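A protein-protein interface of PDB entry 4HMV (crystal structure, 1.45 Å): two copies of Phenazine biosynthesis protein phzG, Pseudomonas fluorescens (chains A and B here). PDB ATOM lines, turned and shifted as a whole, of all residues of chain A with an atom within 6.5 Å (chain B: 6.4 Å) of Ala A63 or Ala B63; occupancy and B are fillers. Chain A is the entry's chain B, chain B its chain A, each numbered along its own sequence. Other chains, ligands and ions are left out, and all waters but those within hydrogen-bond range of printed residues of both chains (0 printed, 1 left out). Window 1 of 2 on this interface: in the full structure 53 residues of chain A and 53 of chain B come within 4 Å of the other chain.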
ATOM      1  N   ALA A  61      22.639  -3.310 -11.849  1.00  0.00           N
ATOM      2  CA  ALA A  61      23.360  -3.443 -13.100  1.00  0.00           C
ATOM      3  C   ALA A  61      22.873  -2.359 -14.048  1.00  0.00           C
ATOM      4  O   ALA A  61      21.761  -2.425 -14.589  1.00  0.00           O
ATOM      5  CB  ALA A  61      23.149  -4.832 -13.689  1.00  0.00           C
ATOM      6  N   LEU A  62      23.717  -1.347 -14.202  1.00  0.00           N
ATOM      7  CA  LEU A  62      23.400  -0.138 -14.923  1.00  0.00           C
ATOM      8  C   LEU A  62      23.967  -0.177 -16.347  1.00  0.00           C
ATOM      9  O   LEU A  62      25.174  -0.337 -16.537  1.00  0.00           O
ATOM     10  CB  LEU A  62      24.003   1.062 -14.181  1.00  0.00           C
ATOM     11  CG  LEU A  62      23.705   2.450 -14.736  1.00  0.00           C
ATOM     12  CD1 LEU A  62      22.233   2.820 -14.464  1.00  0.00           C
ATOM     13  CD2 LEU A  62      24.656   3.473 -14.095  1.00  0.00           C
ATOM     14  N   ALA A  63      23.101   0.001 -17.341  1.00  0.00           N
ATOM     15  CA  ALA A  63      23.571   0.120 -18.718  1.00  0.00           C
ATOM     16  C   ALA A  63      23.968   1.581 -18.904  1.00  0.00           C
ATOM     17  O   ALA A  63      23.101   2.451 -19.011  1.00  0.00           O
ATOM     18  CB  ALA A  63      22.496  -0.302 -19.713  1.00  0.00           C
ATOM     19  N   LEU A  64      25.285   1.826 -18.864  1.00  0.00           N
ATOM     20  CA  LEU A  64      25.863   3.165 -18.810  1.00  0.00           C
ATOM     21  C   LEU A  64      26.322   3.609 -20.185  1.00  0.00           C
ATOM     22  O   LEU A  64      27.145   2.922 -20.821  1.00  0.00           O
ATOM     23  CB  LEU A  64      27.050   3.190 -17.842  1.00  0.00           C
ATOM     24  CG  LEU A  64      27.760   4.549 -17.729  1.00  0.00           C
ATOM     25  CD1 LEU A  64      26.875   5.577 -16.990  1.00  0.00           C
ATOM     26  CD2 LEU A  64      29.122   4.390 -17.049  1.00  0.00           C
ATOM     27  N   ALA A  65      25.814   4.755 -20.630  1.00  0.00           N
ATOM     28  CA  ALA A  65      26.189   5.366 -21.896  1.00  0.00           C
ATOM     29  C   ALA A  65      27.075   6.586 -21.684  1.00  0.00           C
ATOM     30  O   ALA A  65      26.786   7.455 -20.856  1.00  0.00           O
ATOM     31  CB  ALA A  65      24.945   5.768 -22.670  1.00  0.00           C
ATOM     32  N   THR A  75      28.125   2.015 -24.898  1.00  0.00           N
ATOM     33  CA  THR A  75      27.390   1.467 -23.757  1.00  0.00           C
ATOM     34  C   THR A  75      28.075   0.220 -23.225  1.00  0.00           C
ATOM     35  O   THR A  75      28.849  -0.434 -23.939  1.00  0.00           O
ATOM     36  CB  THR A  75      25.943   1.078 -24.123  1.00  0.00           C
ATOM     37  OG1 THR A  75      25.931   0.145 -25.208  1.00  0.00           O
ATOM     38  CG2 THR A  75      25.108   2.289 -24.495  1.00  0.00           C
ATOM     39  N   ARG A  76      27.789  -0.096 -21.962  1.00  0.00           N
ATOM     40  CA  ARG A  76      28.234  -1.316 -21.292  1.00  0.00           C
ATOM     41  C   ARG A  76      27.556  -1.351 -19.930  1.00  0.00           C
ATOM     42  O   ARG A  76      27.065  -0.329 -19.448  1.00  0.00           O
ATOM     43  CB  ARG A  76      29.756  -1.341 -21.075  1.00  0.00           C
ATOM     44  CG  ARG A  76      30.264  -0.444 -19.970  1.00  0.00           C
ATOM     45  CD  ARG A  76      30.088   1.042 -20.238  1.00  0.00           C
ATOM     46  NE  ARG A  76      30.926   1.450 -21.356  1.00  0.00           N
ATOM     47  CZ  ARG A  76      30.867   2.591 -22.013  1.00  0.00           C
ATOM     48  NH1 ARG A  76      31.763   2.825 -22.959  1.00  0.00           N
ATOM     49  NH2 ARG A  76      29.957   3.506 -21.731  1.00  0.00           N
ATOM     50  N   ILE A  77      27.538  -2.523 -19.304  1.00  0.00           N
ATOM     51  CA  ILE A  77      27.054  -2.626 -17.934  1.00  0.00           C
ATOM     52  C   ILE A  77      28.144  -2.241 -16.922  1.00  0.00           C
ATOM     53  O   ILE A  77      29.291  -2.697 -17.043  1.00  0.00           O
ATOM     54  CB  ILE A  77      26.558  -4.074 -17.609  1.00  0.00           C
ATOM     55  CG1 ILE A  77      25.383  -4.477 -18.533  1.00  0.00           C
ATOM     56  CG2 ILE A  77      26.183  -4.198 -16.116  1.00  0.00           C
ATOM     57  CD1 ILE A  77      24.058  -3.693 -18.290  1.00  0.00           C
ATOM     58  N   VAL A  78      27.780  -1.430 -15.933  1.00  0.00           N
ATOM     59  CA  VAL A  78      28.600  -1.266 -14.732  1.00  0.00           C
ATOM     60  C   VAL A  78      27.673  -1.435 -13.537  1.00  0.00           C
ATOM     61  O   VAL A  78      26.452  -1.324 -13.667  1.00  0.00           O
ATOM     62  CB  VAL A  78      29.292   0.112 -14.645  1.00  0.00           C
ATOM     63  CG1 VAL A  78      30.197   0.351 -15.849  1.00  0.00           C
ATOM     64  CG2 VAL A  78      28.266   1.235 -14.481  1.00  0.00           C
ATOM     65  N   SER A 109      24.528   8.848 -19.293  1.00  0.00           N
ATOM     66  CA  SER A 109      23.173   8.396 -18.978  1.00  0.00           C
ATOM     67  C   SER A 109      23.224   6.915 -18.734  1.00  0.00           C
ATOM     68  O   SER A 109      23.878   6.186 -19.465  1.00  0.00           O
ATOM     69  CB  SER A 109      22.227   8.697 -20.145  1.00  0.00           C
ATOM     70  OG  SER A 109      20.906   8.255 -19.880  1.00  0.00           O
ATOM     71  N   GLY A 110      22.478   6.441 -17.739  1.00  0.00           N
ATOM     72  CA  GLY A 110      22.370   5.015 -17.517  1.00  0.00           C
ATOM     73  C   GLY A 110      20.947   4.594 -17.255  1.00  0.00           C
ATOM     74  O   GLY A 110      20.151   5.355 -16.705  1.00  0.00           O
ATOM     75  N   VAL A 111      20.653   3.351 -17.612  1.00  0.00           N
ATOM     76  CA  VAL A 111      19.319   2.789 -17.364  1.00  0.00           C
ATOM     77  C   VAL A 111      19.397   1.485 -16.565  1.00  0.00           C
ATOM     78  O   VAL A 111      20.206   0.594 -16.859  1.00  0.00           O
ATOM     79  CB  VAL A 111      18.506   2.576 -18.678  1.00  0.00           C
ATOM     80  CG1 VAL A 111      19.217   1.752 -19.725  1.00  0.00           C
ATOM     81  CG2 VAL A 111      17.108   1.995 -18.434  1.00  0.00           C
ATOM     82  N   LEU A 112      18.553   1.403 -15.540  1.00  0.00           N
ATOM     83  CA  LEU A 112      18.252   0.185 -14.788  1.00  0.00           C
ATOM     84  C   LEU A 112      16.929  -0.344 -15.325  1.00  0.00           C
ATOM     85  O   LEU A 112      15.999   0.444 -15.566  1.00  0.00           O
ATOM     86  CB  LEU A 112      18.092   0.523 -13.312  1.00  0.00           C
ATOM     87  CG  LEU A 112      19.312   1.130 -12.607  1.00  0.00           C
ATOM     88  CD1 LEU A 112      18.964   1.525 -11.157  1.00  0.00           C
ATOM     89  CD2 LEU A 112      20.536   0.199 -12.605  1.00  0.00           C
ATOM     90  N   ALA B  61      15.686  -7.085 -24.875  1.00  0.00           N
ATOM     91  CA  ALA B  61      15.513  -5.800 -24.220  1.00  0.00           C
ATOM     92  C   ALA B  61      16.843  -5.048 -24.296  1.00  0.00           C
ATOM     93  O   ALA B  61      17.770  -5.319 -23.549  1.00  0.00           O
ATOM     94  CB  ALA B  61      15.086  -6.011 -22.771  1.00  0.00           C
ATOM     95  N   LEU B  62      16.908  -4.107 -25.224  1.00  0.00           N
ATOM     96  CA  LEU B  62      18.106  -3.374 -25.555  1.00  0.00           C
ATOM     97  C   LEU B  62      18.153  -2.032 -24.845  1.00  0.00           C
ATOM     98  O   LEU B  62      17.248  -1.211 -24.994  1.00  0.00           O
ATOM     99  CB  LEU B  62      18.159  -3.154 -27.091  1.00  0.00           C
ATOM    100  CG  LEU B  62      19.429  -2.478 -27.615  1.00  0.00           C
ATOM    101  CD1 LEU B  62      20.624  -3.394 -27.527  1.00  0.00           C
ATOM    102  CD2 LEU B  62      19.188  -2.005 -29.054  1.00  0.00           C
ATOM    103  N   ALA B  63      19.210  -1.783 -24.070  1.00  0.00           N
ATOM    104  CA  ALA B  63      19.414  -0.470 -23.488  1.00  0.00           C
ATOM    105  C   ALA B  63      20.069   0.399 -24.539  1.00  0.00           C
ATOM    106  O   ALA B  63      21.269   0.255 -24.816  1.00  0.00           O
ATOM    107  CB  ALA B  63      20.261  -0.570 -22.226  1.00  0.00           C
ATOM    108  N   LEU B  64      19.261   1.273 -25.159  1.00  0.00           N
ATOM    109  CA  LEU B  64      19.659   2.034 -26.344  1.00  0.00           C
ATOM    110  C   LEU B  64      20.040   3.457 -25.969  1.00  0.00           C
ATOM    111  O   LEU B  64      19.231   4.173 -25.364  1.00  0.00           O
ATOM    112  CB  LEU B  64      18.504   2.106 -27.328  1.00  0.00           C
ATOM    113  CG  LEU B  64      18.760   2.915 -28.599  1.00  0.00           C
ATOM    114  CD1 LEU B  64      19.692   2.172 -29.528  1.00  0.00           C
ATOM    115  CD2 LEU B  64      17.413   3.240 -29.260  1.00  0.00           C
ATOM    116  N   ALA B  65      21.254   3.847 -26.346  1.00  0.00           N
ATOM    117  CA  ALA B  65      21.787   5.179 -26.104  1.00  0.00           C
ATOM    118  C   ALA B  65      21.828   5.987 -27.391  1.00  0.00           C
ATOM    119  O   ALA B  65      22.271   5.507 -28.422  1.00  0.00           O
ATOM    120  CB  ALA B  65      23.227   5.080 -25.531  1.00  0.00           C
ATOM    121  N   THR B  75      19.323   7.400 -22.470  1.00  0.00           N
ATOM    122  CA  THR B  75      19.119   5.971 -22.553  1.00  0.00           C
ATOM    123  C   THR B  75      17.688   5.572 -22.233  1.00  0.00           C
ATOM    124  O   THR B  75      16.945   6.312 -21.571  1.00  0.00           O
ATOM    125  CB  THR B  75      20.045   5.179 -21.601  1.00  0.00           C
ATOM    126  OG1 THR B  75      19.832   5.606 -20.238  1.00  0.00           O
ATOM    127  CG2 THR B  75      21.519   5.347 -21.953  1.00  0.00           C
ATOM    128  N   ARG B  76      17.316   4.386 -22.702  1.00  0.00           N
ATOM    129  CA  ARG B  76      16.030   3.760 -22.382  1.00  0.00           C
ATOM    130  C   ARG B  76      16.057   2.351 -22.955  1.00  0.00           C
ATOM    131  O   ARG B  76      16.871   2.052 -23.824  1.00  0.00           O
ATOM    132  CB  ARG B  76      14.843   4.528 -23.000  1.00  0.00           C
ATOM    133  CG  ARG B  76      14.686   4.337 -24.513  1.00  0.00           C
ATOM    134  CD  ARG B  76      15.794   4.989 -25.323  1.00  0.00           C
ATOM    135  NE  ARG B  76      15.800   6.432 -25.169  1.00  0.00           N
ATOM    136  CZ  ARG B  76      16.762   7.242 -25.580  1.00  0.00           C
ATOM    137  NH1 ARG B  76      16.577   8.543 -25.475  1.00  0.00           N
ATOM    138  NH2 ARG B  76      17.883   6.775 -26.096  1.00  0.00           N
ATOM    139  N   ILE B  77      15.138   1.488 -22.505  1.00  0.00           N
ATOM    140  CA  ILE B  77      14.991   0.175 -23.103  1.00  0.00           C
ATOM    141  C   ILE B  77      14.092   0.253 -24.356  1.00  0.00           C
ATOM    142  O   ILE B  77      13.035   0.885 -24.347  1.00  0.00           O
ATOM    143  CB  ILE B  77      14.352  -0.828 -22.117  1.00  0.00           C
ATOM    144  CG1 ILE B  77      15.225  -0.977 -20.865  1.00  0.00           C
ATOM    145  CG2 ILE B  77      14.166  -2.195 -22.781  1.00  0.00           C
ATOM    146  CD1 ILE B  77      16.641  -1.554 -21.070  1.00  0.00           C
ATOM    147  N   VAL B  78      14.520  -0.415 -25.428  1.00  0.00           N
ATOM    148  CA  VAL B  78      13.660  -0.724 -26.571  1.00  0.00           C
ATOM    149  C   VAL B  78      13.810  -2.215 -26.872  1.00  0.00           C
ATOM    150  O   VAL B  78      14.792  -2.854 -26.475  1.00  0.00           O
ATOM    151  CB  VAL B  78      13.974   0.132 -27.831  1.00  0.00           C
ATOM    152  CG1 VAL B  78      13.785   1.623 -27.534  1.00  0.00           C
ATOM    153  CG2 VAL B  78      15.376  -0.189 -28.415  1.00  0.00           C
ATOM    154  N   SER B 109      24.259   3.450 -29.622  1.00  0.00           N
ATOM    155  CA  SER B 109      24.847   2.238 -29.101  1.00  0.00           C
ATOM    156  C   SER B 109      23.821   1.584 -28.207  1.00  0.00           C
ATOM    157  O   SER B 109      23.096   2.289 -27.489  1.00  0.00           O
ATOM    158  CB  SER B 109      26.082   2.593 -28.273  1.00  0.00           C
ATOM    159  OG  SER B 109      26.615   1.437 -27.673  1.00  0.00           O
ATOM    160  N   GLY B 110      23.768   0.273 -28.228  1.00  0.00           N
ATOM    161  CA  GLY B 110      22.900  -0.451 -27.325  1.00  0.00           C
ATOM    162  C   GLY B 110      23.582  -1.642 -26.703  1.00  0.00           C
ATOM    163  O   GLY B 110      24.465  -2.249 -27.289  1.00  0.00           O
ATOM    164  N   VAL B 111      23.136  -1.995 -25.496  1.00  0.00           N
ATOM    165  CA  VAL B 111      23.652  -3.179 -24.835  1.00  0.00           C
ATOM    166  C   VAL B 111      22.517  -4.119 -24.452  1.00  0.00           C
ATOM    167  O   VAL B 111      21.486  -3.690 -23.888  1.00  0.00           O
ATOM    168  CB  VAL B 111      24.533  -2.846 -23.612  1.00  0.00           C
ATOM    169  CG1 VAL B 111      23.864  -1.935 -22.609  1.00  0.00           C
ATOM    170  CG2 VAL B 111      25.067  -4.109 -22.931  1.00  0.00           C
ATOM    171  N   LEU B 112      22.747  -5.402 -24.749  1.00  0.00           N
ATOM    172  CA  LEU B 112      21.940  -6.500 -24.252  1.00  0.00           C
ATOM    173  C   LEU B 112      22.717  -7.139 -23.107  1.00  0.00           C
ATOM    174  O   LEU B 112      23.930  -7.347 -23.220  1.00  0.00           O
ATOM    175  CB  LEU B 112      21.695  -7.532 -25.347  1.00  0.00           C
ATOM    176  CG  LEU B 112      20.961  -7.094 -26.602  1.00  0.00           C
ATOM    177  CD1 LEU B 112      21.007  -8.203 -27.665  1.00  0.00           C
ATOM    178  CD2 LEU B 112      19.507  -6.735 -26.286  1.00  0.00           C
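N of Ala B63 sits at hydrogen-bond distance from O of Val B111, at 3.0 Å.
N of Ala B65 lies within hydrogen-bond range of O of Ser B109 (2.7 Å).
O of Ala A63 lies within hydrogen-bond range of N of Val A111.
O of Ser A109 is in hydrogen-bond range of N of Ala A65.
Hydrophobic or aromatic side chains of chain A within 4 Å of the printed part of chain B: Ala A63, Ala A65 and Val A111.
Printed residues of chain B that touch a printed residue of chain A: Ala B63, Ala B65, Thr B75, Ser B109, Gly B110 and Val B111.
Hydrophobic or aromatic side chains of chain B that line the printed part of chain A: Ala B63, Ala B65 and Val B111.
Along chain B the printed residues that touch a printed residue of chain A span positions 63 to 111.
Among the printed residues, 12 pairs touch across the chains.
Among the printed residues, no Asp or Glu carboxylate lies within 4 Å of a Lys or Arg side-chain nitrogen of the other chain.
Ala B63 touches its own counterpart, Ala A63.
Ala A65 touches its own counterpart, Ala B65.
Ala A65 touches Thr B75, and with the chains exchanged Thr A75 touches Ala B65.
Thr A75 touches Gly B110, and with the chains exchanged Gly A110 touches Thr B75.
Positions printed for both chains: 61, 62, 63, 64, 65, 75, 76, 77, 78, 109, 110, 111 and 112.
Of the 12 pairs that touch across the chains among the printed residues, 12 have their exchanged pair printed and touching as well.
Ala A63 touches Ala B63.
Val B111 touches Ala A63.
Ala B65 touches Ala A65.
Thr B75 touches Ala A65.
Ala B65 touches Thr A75.
OG1 of Thr A75 touches N of Val B111, 3.5 Å away.
OG1 of Thr B75 touches C of Gly A110 (3.3 Å).
Val A111 touches Ala B63.
Thr B75 touches Val A111 (OG1 to N, 3.6 Å).
Ala A63 touches two residues of chain B.
Printed residues of chain B within 4 Å of Ala A65: Ala B65 (3.4 Å) and Thr B75 (3.5 Å).
Printed residues of chain B within 4 Å of Ser A109: Thr B75 (2.9 Å).
Of the printed residues of chain B, Val A111 touches Ala B63 (3.6 Å) and Thr B75 (3.6 Å).
Ala B61 touches none of the printed residues of chain A.
Ala B63 touches two residues of chain A.
Leu B64 touches none of the printed residues of chain A.
The nearest residue of chain B that does not touch Ala A63 is Thr B75 (4.4 Å).
OG of Ser A109 lies within hydrogen-bond range of OG1 of Thr B75 (2.9 Å).
The side-chain hydroxyl (OG) of Ser B109 lies within hydrogen-bond range of the side-chain hydroxyl (OG1) of Thr A75, 2.9 Å away.
O of Gly B110 sits close to OG1 of Thr A75 (3.5 Å).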
